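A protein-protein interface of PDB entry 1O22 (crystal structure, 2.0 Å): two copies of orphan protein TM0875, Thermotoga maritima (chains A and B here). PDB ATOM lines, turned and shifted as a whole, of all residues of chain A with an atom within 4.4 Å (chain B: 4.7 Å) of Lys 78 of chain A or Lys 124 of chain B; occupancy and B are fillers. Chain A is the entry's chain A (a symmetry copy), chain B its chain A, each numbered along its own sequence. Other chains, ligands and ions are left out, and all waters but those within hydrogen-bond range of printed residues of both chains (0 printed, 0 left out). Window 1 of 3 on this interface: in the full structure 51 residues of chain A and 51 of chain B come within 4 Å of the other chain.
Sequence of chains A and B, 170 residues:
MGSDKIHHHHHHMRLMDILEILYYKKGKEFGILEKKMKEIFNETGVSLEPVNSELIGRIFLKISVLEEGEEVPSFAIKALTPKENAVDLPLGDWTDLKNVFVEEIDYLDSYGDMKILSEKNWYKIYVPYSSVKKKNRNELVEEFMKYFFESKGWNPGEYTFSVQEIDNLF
NZ of Lys 124 of chain B lies within salt-bridge range of OE2 of Glu 104 of chain A (2.7 Å).
The side-chain carboxylate (OE1) of Glu 103 of chain A sits close to the side-chain hydroxyl (OH) of Tyr 126 of chain B.
N of Ile 77 of chain B sits at hydrogen-bond distance from O of Ala 79 of chain A (2.8 Å).
O of Ile 77 of chain A lies close to O of Ile 77 of chain B (3.4 Å).
The side-chain amino group of Lys 124 of chain B is in salt-bridge range of the side-chain carboxylate of Glu 103 of chain A, at 3.3 Å.
The side-chain carboxylate of Glu 104 of chain A is in salt-bridge range of the side-chain amino group of Lys 78 of chain A, 2.8 Å away.
The backbone NH of Leu 117 of chain B lies within hydrogen-bond range of the backbone carbonyl oxygen of Lys 124 of chain B (2.9 Å).
N of Tyr 126 of chain B lies within hydrogen-bond range of O of Lys 115 of chain B (2.8 Å).
O of Lys 78 of chain A sits at hydrogen-bond distance from N of Glu 103 of chain A (2.8 Å).
Among the printed residues, merely in contact across the chains: Ile 77 of chain A with Lys 78 of chain B (3.4 Å), Lys 78 of chain A with Ile 77 of chain B (3.4 Å) and Lys 78 of chain A with Lys 124 of chain B (3.8 Å).
Of the printed residues of chain B, Lys 78 of chain A touches Ile 77 (3.4 Å) and Lys 124 (3.8 Å).
Of the printed residues of chain B, Glu 103 of chain A touches Lys 124 (3.3 Å) and Tyr 126 (2.2 Å).
Printed residues of chain B within 4 Å of Glu 104 of chain A: Lys 124.
Lys 124 of chain B touches just these residues of chain A: Lys 78 (3.8 Å), Glu 103 (3.3 Å) and Glu 104 (2.7 Å).
Of the printed residues of chain A, Tyr 126 of chain B touches Glu 103.
Of the 12 printed residues of chain B, 4 touch a printed residue of chain A.
Hydrophobic or aromatic side chains of chain B that line the printed part of chain A: Ile 77 and Tyr 126.
Of the 8 printed residues of chain A, 5 touch a printed residue of chain B.
Ile 77 of chain B touches its own counterpart, Ile 77 of chain A.
Ile 77 of chain A touches Lys 78 of chain B, and with the chains exchanged Lys 78 of chain A touches Ile 77 of chain B.
Positions printed for both chains: 77 and 78.
Of the 8 pairs that touch across the chains among the printed residues, 3 have their exchanged pair printed and touching as well.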
ATOM      1  N   ALA A  76      12.070 -11.378   0.318  1.00  0.00           N
ATOM      2  CA  ALA A  76      11.839 -11.548   1.735  1.00  0.00           C
ATOM      3  C   ALA A  76      11.338 -12.985   1.908  1.00  0.00           C
ATOM      4  O   ALA A  76      10.450 -13.428   1.173  1.00  0.00           O
ATOM      5  CB  ALA A  76      10.813 -10.557   2.221  1.00  0.00           C
ATOM      6  N   ILE A  77      11.973 -13.727   2.804  1.00  0.00           N
ATOM      7  CA  ILE A  77      11.617 -15.114   3.093  1.00  0.00           C
ATOM      8  C   ILE A  77      11.031 -15.198   4.516  1.00  0.00           C
ATOM      9  O   ILE A  77      11.627 -14.685   5.472  1.00  0.00           O
ATOM     10  CB  ILE A  77      12.860 -15.982   2.993  1.00  0.00           C
ATOM     11  CG1 ILE A  77      13.528 -15.809   1.624  1.00  0.00           C
ATOM     12  CG2 ILE A  77      12.505 -17.454   3.229  1.00  0.00           C
ATOM     13  CD1 ILE A  77      14.912 -16.350   1.568  1.00  0.00           C
ATOM     14  N   LYS A  78       9.848 -15.783   4.658  1.00  0.00           N
ATOM     15  CA  LYS A  78       9.376 -16.215   5.990  1.00  0.00           C
ATOM     16  C   LYS A  78       9.729 -17.672   6.179  1.00  0.00           C
ATOM     17  O   LYS A  78       9.285 -18.533   5.433  1.00  0.00           O
ATOM     18  CB  LYS A  78       7.882 -15.997   6.155  1.00  0.00           C
ATOM     19  CG  LYS A  78       7.515 -14.498   6.160  1.00  0.00           C
ATOM     20  CD  LYS A  78       6.006 -14.273   6.200  1.00  0.00           C
ATOM     21  CE  LYS A  78       5.631 -12.992   5.460  1.00  0.00           C
ATOM     22  NZ  LYS A  78       4.173 -12.727   5.523  1.00  0.00           N
ATOM     23  N   ALA A  79      10.608 -17.915   7.125  1.00  0.00           N
ATOM     24  CA  ALA A  79      11.064 -19.254   7.475  1.00  0.00           C
ATOM     25  C   ALA A  79      10.618 -19.600   8.903  1.00  0.00           C
ATOM     26  O   ALA A  79      10.520 -18.738   9.760  1.00  0.00           O
ATOM     27  CB  ALA A  79      12.573 -19.299   7.383  1.00  0.00           C
ATOM     28  N   PHE A 101      11.980 -24.269   7.621  1.00  0.00           N
ATOM     29  CA  PHE A 101      10.834 -24.401   6.753  1.00  0.00           C
ATOM     30  C   PHE A 101      10.488 -23.064   6.090  1.00  0.00           C
ATOM     31  O   PHE A 101      10.143 -22.102   6.763  1.00  0.00           O
ATOM     32  CB  PHE A 101       9.655 -24.932   7.546  1.00  0.00           C
ATOM     33  CG  PHE A 101       8.449 -25.225   6.724  1.00  0.00           C
ATOM     34  CD1 PHE A 101       8.312 -26.438   6.112  1.00  0.00           C
ATOM     35  CD2 PHE A 101       7.437 -24.289   6.593  1.00  0.00           C
ATOM     36  CE1 PHE A 101       7.185 -26.743   5.368  1.00  0.00           C
ATOM     37  CE2 PHE A 101       6.299 -24.575   5.854  1.00  0.00           C
ATOM     38  CZ  PHE A 101       6.172 -25.811   5.239  1.00  0.00           C
ATOM     39  N   VAL A 102      10.563 -23.017   4.759  1.00  0.00           N
ATOM     40  CA  VAL A 102      10.157 -21.835   4.011  1.00  0.00           C
ATOM     41  C   VAL A 102       8.680 -21.770   3.798  1.00  0.00           C
ATOM     42  O   VAL A 102       8.111 -22.593   3.122  1.00  0.00           O
ATOM     43  CB  VAL A 102      10.842 -21.778   2.670  1.00  0.00           C
ATOM     44  CG1 VAL A 102      10.396 -20.494   1.888  1.00  0.00           C
ATOM     45  CG2 VAL A 102      12.320 -21.831   2.846  1.00  0.00           C
ATOM     46  N   GLU A 103       8.041 -20.779   4.377  1.00  0.00           N
ATOM     47  CA  GLU A 103       6.598 -20.677   4.332  1.00  0.00           C
ATOM     48  C   GLU A 103       6.102 -19.687   3.260  1.00  0.00           C
ATOM     49  O   GLU A 103       5.071 -19.906   2.621  1.00  0.00           O
ATOM     50  CB  GLU A 103       6.118 -20.234   5.704  1.00  0.00           C
ATOM     51  CG  GLU A 103       4.621 -20.295   5.853  1.00  0.00           C
ATOM     52  CD  GLU A 103       4.188 -19.668   7.137  1.00  0.00           C
ATOM     53  OE1 GLU A 103       4.685 -18.564   7.448  1.00  0.00           O
ATOM     54  OE2 GLU A 103       3.369 -20.287   7.830  1.00  0.00           O
ATOM     55  N   GLU A 104       6.827 -18.590   3.094  1.00  0.00           N
ATOM     56  CA  GLU A 104       6.455 -17.526   2.153  1.00  0.00           C
ATOM     57  C   GLU A 104       7.726 -16.903   1.543  1.00  0.00           C
ATOM     58  O   GLU A 104       8.763 -16.778   2.208  1.00  0.00           O
ATOM     59  CB  GLU A 104       5.604 -16.426   2.848  1.00  0.00           C
ATOM     60  CG  GLU A 104       4.363 -16.940   3.592  1.00  0.00           C
ATOM     61  CD  GLU A 104       3.415 -15.835   4.081  1.00  0.00           C
ATOM     62  OE1 GLU A 104       3.539 -14.673   3.621  1.00  0.00           O
ATOM     63  OE2 GLU A 104       2.524 -16.137   4.924  1.00  0.00           O
ATOM     64  N   LYS B  62      -5.018 -18.487   9.111  1.00  0.00           N
ATOM     65  CA  LYS B  62      -4.555 -19.534   8.214  1.00  0.00           C
ATOM     66  C   LYS B  62      -4.135 -20.740   9.051  1.00  0.00           C
ATOM     67  O   LYS B  62      -3.408 -20.617  10.045  1.00  0.00           O
ATOM     68  CB  LYS B  62      -3.430 -19.003   7.344  1.00  0.00           C
ATOM     69  CG  LYS B  62      -2.632 -20.050   6.539  1.00  0.00           C
ATOM     70  CD  LYS B  62      -3.277 -20.505   5.230  1.00  0.00           C
ATOM     71  CE  LYS B  62      -2.425 -21.598   4.542  1.00  0.00           C
ATOM     72  N   ILE B  77      11.036 -16.575  11.394  1.00  0.00           N
ATOM     73  CA  ILE B  77      12.130 -15.682  11.021  1.00  0.00           C
ATOM     74  C   ILE B  77      11.771 -14.966   9.705  1.00  0.00           C
ATOM     75  O   ILE B  77      11.374 -15.612   8.727  1.00  0.00           O
ATOM     76  CB  ILE B  77      13.401 -16.495  10.838  1.00  0.00           C
ATOM     77  CG1 ILE B  77      13.700 -17.314  12.098  1.00  0.00           C
ATOM     78  CG2 ILE B  77      14.582 -15.574  10.510  1.00  0.00           C
ATOM     79  CD1 ILE B  77      14.718 -18.379  11.884  1.00  0.00           C
ATOM     80  N   LYS B  78      11.847 -13.641   9.687  1.00  0.00           N
ATOM     81  CA  LYS B  78      11.862 -12.904   8.407  1.00  0.00           C
ATOM     82  C   LYS B  78      13.299 -12.643   8.016  1.00  0.00           C
ATOM     83  O   LYS B  78      14.038 -11.979   8.729  1.00  0.00           O
ATOM     84  CB  LYS B  78      11.084 -11.602   8.498  1.00  0.00           C
ATOM     85  CG  LYS B  78       9.574 -11.846   8.704  1.00  0.00           C
ATOM     86  CD  LYS B  78       8.803 -10.547   8.921  1.00  0.00           C
ATOM     87  CE  LYS B  78       7.606 -10.776   9.839  1.00  0.00           C
ATOM     88  NZ  LYS B  78       6.814  -9.536  10.029  1.00  0.00           N
ATOM     89  N   LYS B 115       0.633 -24.247  17.696  1.00  0.00           N
ATOM     90  CA  LYS B 115       1.493 -23.060  17.725  1.00  0.00           C
ATOM     91  C   LYS B 115       0.866 -21.931  16.900  1.00  0.00           C
ATOM     92  O   LYS B 115       0.349 -22.129  15.833  1.00  0.00           O
ATOM     93  CB  LYS B 115       2.882 -23.370  17.197  1.00  0.00           C
ATOM     94  CG  LYS B 115       3.602 -24.391  17.953  1.00  0.00           C
ATOM     95  CD  LYS B 115       3.743 -24.083  19.458  1.00  0.00           C
ATOM     96  CE  LYS B 115       4.995 -23.391  19.777  1.00  0.00           C
ATOM     97  NZ  LYS B 115       6.113 -24.360  19.776  1.00  0.00           N
ATOM     98  N   ILE B 116       0.951 -20.732  17.420  1.00  0.00           N
ATOM     99  CA  ILE B 116       0.189 -19.604  16.904  1.00  0.00           C
ATOM    100  C   ILE B 116       1.142 -18.430  16.736  1.00  0.00           C
ATOM    101  O   ILE B 116       1.824 -18.022  17.687  1.00  0.00           O
ATOM    102  CB  ILE B 116      -0.933 -19.216  17.892  1.00  0.00           C
ATOM    103  CG1 ILE B 116      -1.893 -20.385  18.108  1.00  0.00           C
ATOM    104  CG2 ILE B 116      -1.629 -17.942  17.436  1.00  0.00           C
ATOM    105  CD1 ILE B 116      -2.303 -20.515  19.477  1.00  0.00           C
ATOM    106  N   LEU B 117       1.165 -17.926  15.515  1.00  0.00           N
ATOM    107  CA  LEU B 117       1.872 -16.723  15.117  1.00  0.00           C
ATOM    108  C   LEU B 117       0.839 -15.619  14.905  1.00  0.00           C
ATOM    109  O   LEU B 117      -0.110 -15.780  14.148  1.00  0.00           O
ATOM    110  CB  LEU B 117       2.582 -16.960  13.800  1.00  0.00           C
ATOM    111  CG  LEU B 117       3.520 -15.874  13.277  1.00  0.00           C
ATOM    112  CD1 LEU B 117       4.640 -15.507  14.276  1.00  0.00           C
ATOM    113  CD2 LEU B 117       4.103 -16.390  11.970  1.00  0.00           C
ATOM    114  N   GLU B 119       0.126 -11.555  13.965  1.00  0.00           N
ATOM    115  CA  GLU B 119       0.489 -10.223  13.525  1.00  0.00           C
ATOM    116  C   GLU B 119      -0.776  -9.368  13.438  1.00  0.00           C
ATOM    117  O   GLU B 119      -1.549  -9.543  12.539  1.00  0.00           O
ATOM    118  CB  GLU B 119       1.262 -10.305  12.187  1.00  0.00           C
ATOM    119  CG  GLU B 119       0.615 -11.166  11.099  1.00  0.00           C
ATOM    120  CD  GLU B 119       1.167 -12.594  11.008  1.00  0.00           C
ATOM    121  OE1 GLU B 119       0.355 -13.576  11.115  1.00  0.00           O
ATOM    122  OE2 GLU B 119       2.404 -12.725  10.815  1.00  0.00           O
ATOM    123  N   TRP B 122      -4.148 -10.812  12.060  1.00  0.00           N
ATOM    124  CA  TRP B 122      -3.847 -11.941  11.160  1.00  0.00           C
ATOM    125  C   TRP B 122      -3.143 -13.034  11.967  1.00  0.00           C
ATOM    126  O   TRP B 122      -2.141 -12.763  12.612  1.00  0.00           O
ATOM    127  CB  TRP B 122      -2.925 -11.493  10.006  1.00  0.00           C
ATOM    128  CG  TRP B 122      -3.647 -10.598   9.035  1.00  0.00           C
ATOM    129  CD1 TRP B 122      -3.952  -9.280   9.205  1.00  0.00           C
ATOM    130  CD2 TRP B 122      -4.175 -10.966   7.744  1.00  0.00           C
ATOM    131  NE1 TRP B 122      -4.633  -8.799   8.106  1.00  0.00           N
ATOM    132  CE2 TRP B 122      -4.781  -9.809   7.191  1.00  0.00           C
ATOM    133  CE3 TRP B 122      -4.190 -12.155   6.992  1.00  0.00           C
ATOM    134  CZ2 TRP B 122      -5.398  -9.808   5.930  1.00  0.00           C
ATOM    135  CZ3 TRP B 122      -4.815 -12.146   5.733  1.00  0.00           C
ATOM    136  CH2 TRP B 122      -5.404 -10.984   5.226  1.00  0.00           C
ATOM    137  N   TYR B 123      -3.661 -14.249  11.918  1.00  0.00           N
ATOM    138  CA  TYR B 123      -3.143 -15.330  12.742  1.00  0.00           C
ATOM    139  C   TYR B 123      -2.810 -16.498  11.847  1.00  0.00           C
ATOM    140  O   TYR B 123      -3.493 -16.724  10.894  1.00  0.00           O
ATOM    141  CB  TYR B 123      -4.170 -15.759  13.788  1.00  0.00           C
ATOM    142  CG  TYR B 123      -4.413 -14.720  14.848  1.00  0.00           C
ATOM    143  CD1 TYR B 123      -3.786 -14.798  16.082  1.00  0.00           C
ATOM    144  CD2 TYR B 123      -5.292 -13.680  14.628  1.00  0.00           C
ATOM    145  CE1 TYR B 123      -4.029 -13.855  17.062  1.00  0.00           C
ATOM    146  CE2 TYR B 123      -5.541 -12.733  15.595  1.00  0.00           C
ATOM    147  CZ  TYR B 123      -4.906 -12.808  16.805  1.00  0.00           C
ATOM    148  OH  TYR B 123      -5.152 -11.850  17.784  1.00  0.00           O
ATOM    149  N   LYS B 124      -1.749 -17.217  12.188  1.00  0.00           N
ATOM    150  CA  LYS B 124      -1.372 -18.455  11.500  1.00  0.00           C
ATOM    151  C   LYS B 124      -1.187 -19.496  12.584  1.00  0.00           C
ATOM    152  O   LYS B 124      -0.480 -19.252  13.554  1.00  0.00           O
ATOM    153  CB  LYS B 124      -0.051 -18.263  10.759  1.00  0.00           C
ATOM    154  CG  LYS B 124      -0.063 -17.244   9.636  1.00  0.00           C
ATOM    155  CD  LYS B 124       1.351 -17.005   9.152  1.00  0.00           C
ATOM    156  CE  LYS B 124       1.415 -16.240   7.846  1.00  0.00           C
ATOM    157  NZ  LYS B 124       2.836 -15.816   7.599  1.00  0.00           N
ATOM    158  N   ILE B 125      -1.873 -20.623  12.458  1.00  0.00           N
ATOM    159  CA  ILE B 125      -1.705 -21.695  13.386  1.00  0.00           C
ATOM    160  C   ILE B 125      -1.110 -22.897  12.718  1.00  0.00           C
ATOM    161  O   ILE B 125      -1.313 -23.133  11.537  1.00  0.00           O
ATOM    162  CB  ILE B 125      -3.034 -22.025  14.095  1.00  0.00           C
ATOM    163  CG1 ILE B 125      -4.062 -22.580  13.145  1.00  0.00           C
ATOM    164  CG2 ILE B 125      -3.575 -20.737  14.837  1.00  0.00           C
ATOM    165  CD1 ILE B 125      -5.250 -23.178  13.903  1.00  0.00           C
ATOM    166  N   TYR B 126      -0.314 -23.609  13.493  1.00  0.00           N
ATOM    167  CA  TYR B 126       0.449 -24.756  13.030  1.00  0.00           C
ATOM    168  C   TYR B 126       0.128 -25.871  13.961  1.00  0.00           C
ATOM    169  O   TYR B 126       0.191 -25.703  15.188  1.00  0.00           O
ATOM    170  CB  TYR B 126       1.944 -24.458  13.087  1.00  0.00           C
ATOM    171  CG  TYR B 126       2.298 -23.284  12.255  1.00  0.00           C
ATOM    172  CD1 TYR B 126       2.655 -23.434  10.922  1.00  0.00           C
ATOM    173  CD2 TYR B 126       2.262 -21.995  12.799  1.00  0.00           C
ATOM    174  CE1 TYR B 126       2.955 -22.313  10.147  1.00  0.00           C
ATOM    175  CE2 TYR B 126       2.559 -20.927  12.073  1.00  0.00           C
ATOM    176  CZ  TYR B 126       2.915 -21.074  10.740  1.00  0.00           C
ATOM    177  OH  TYR B 126       3.198 -19.934  10.044  1.00  0.00           O
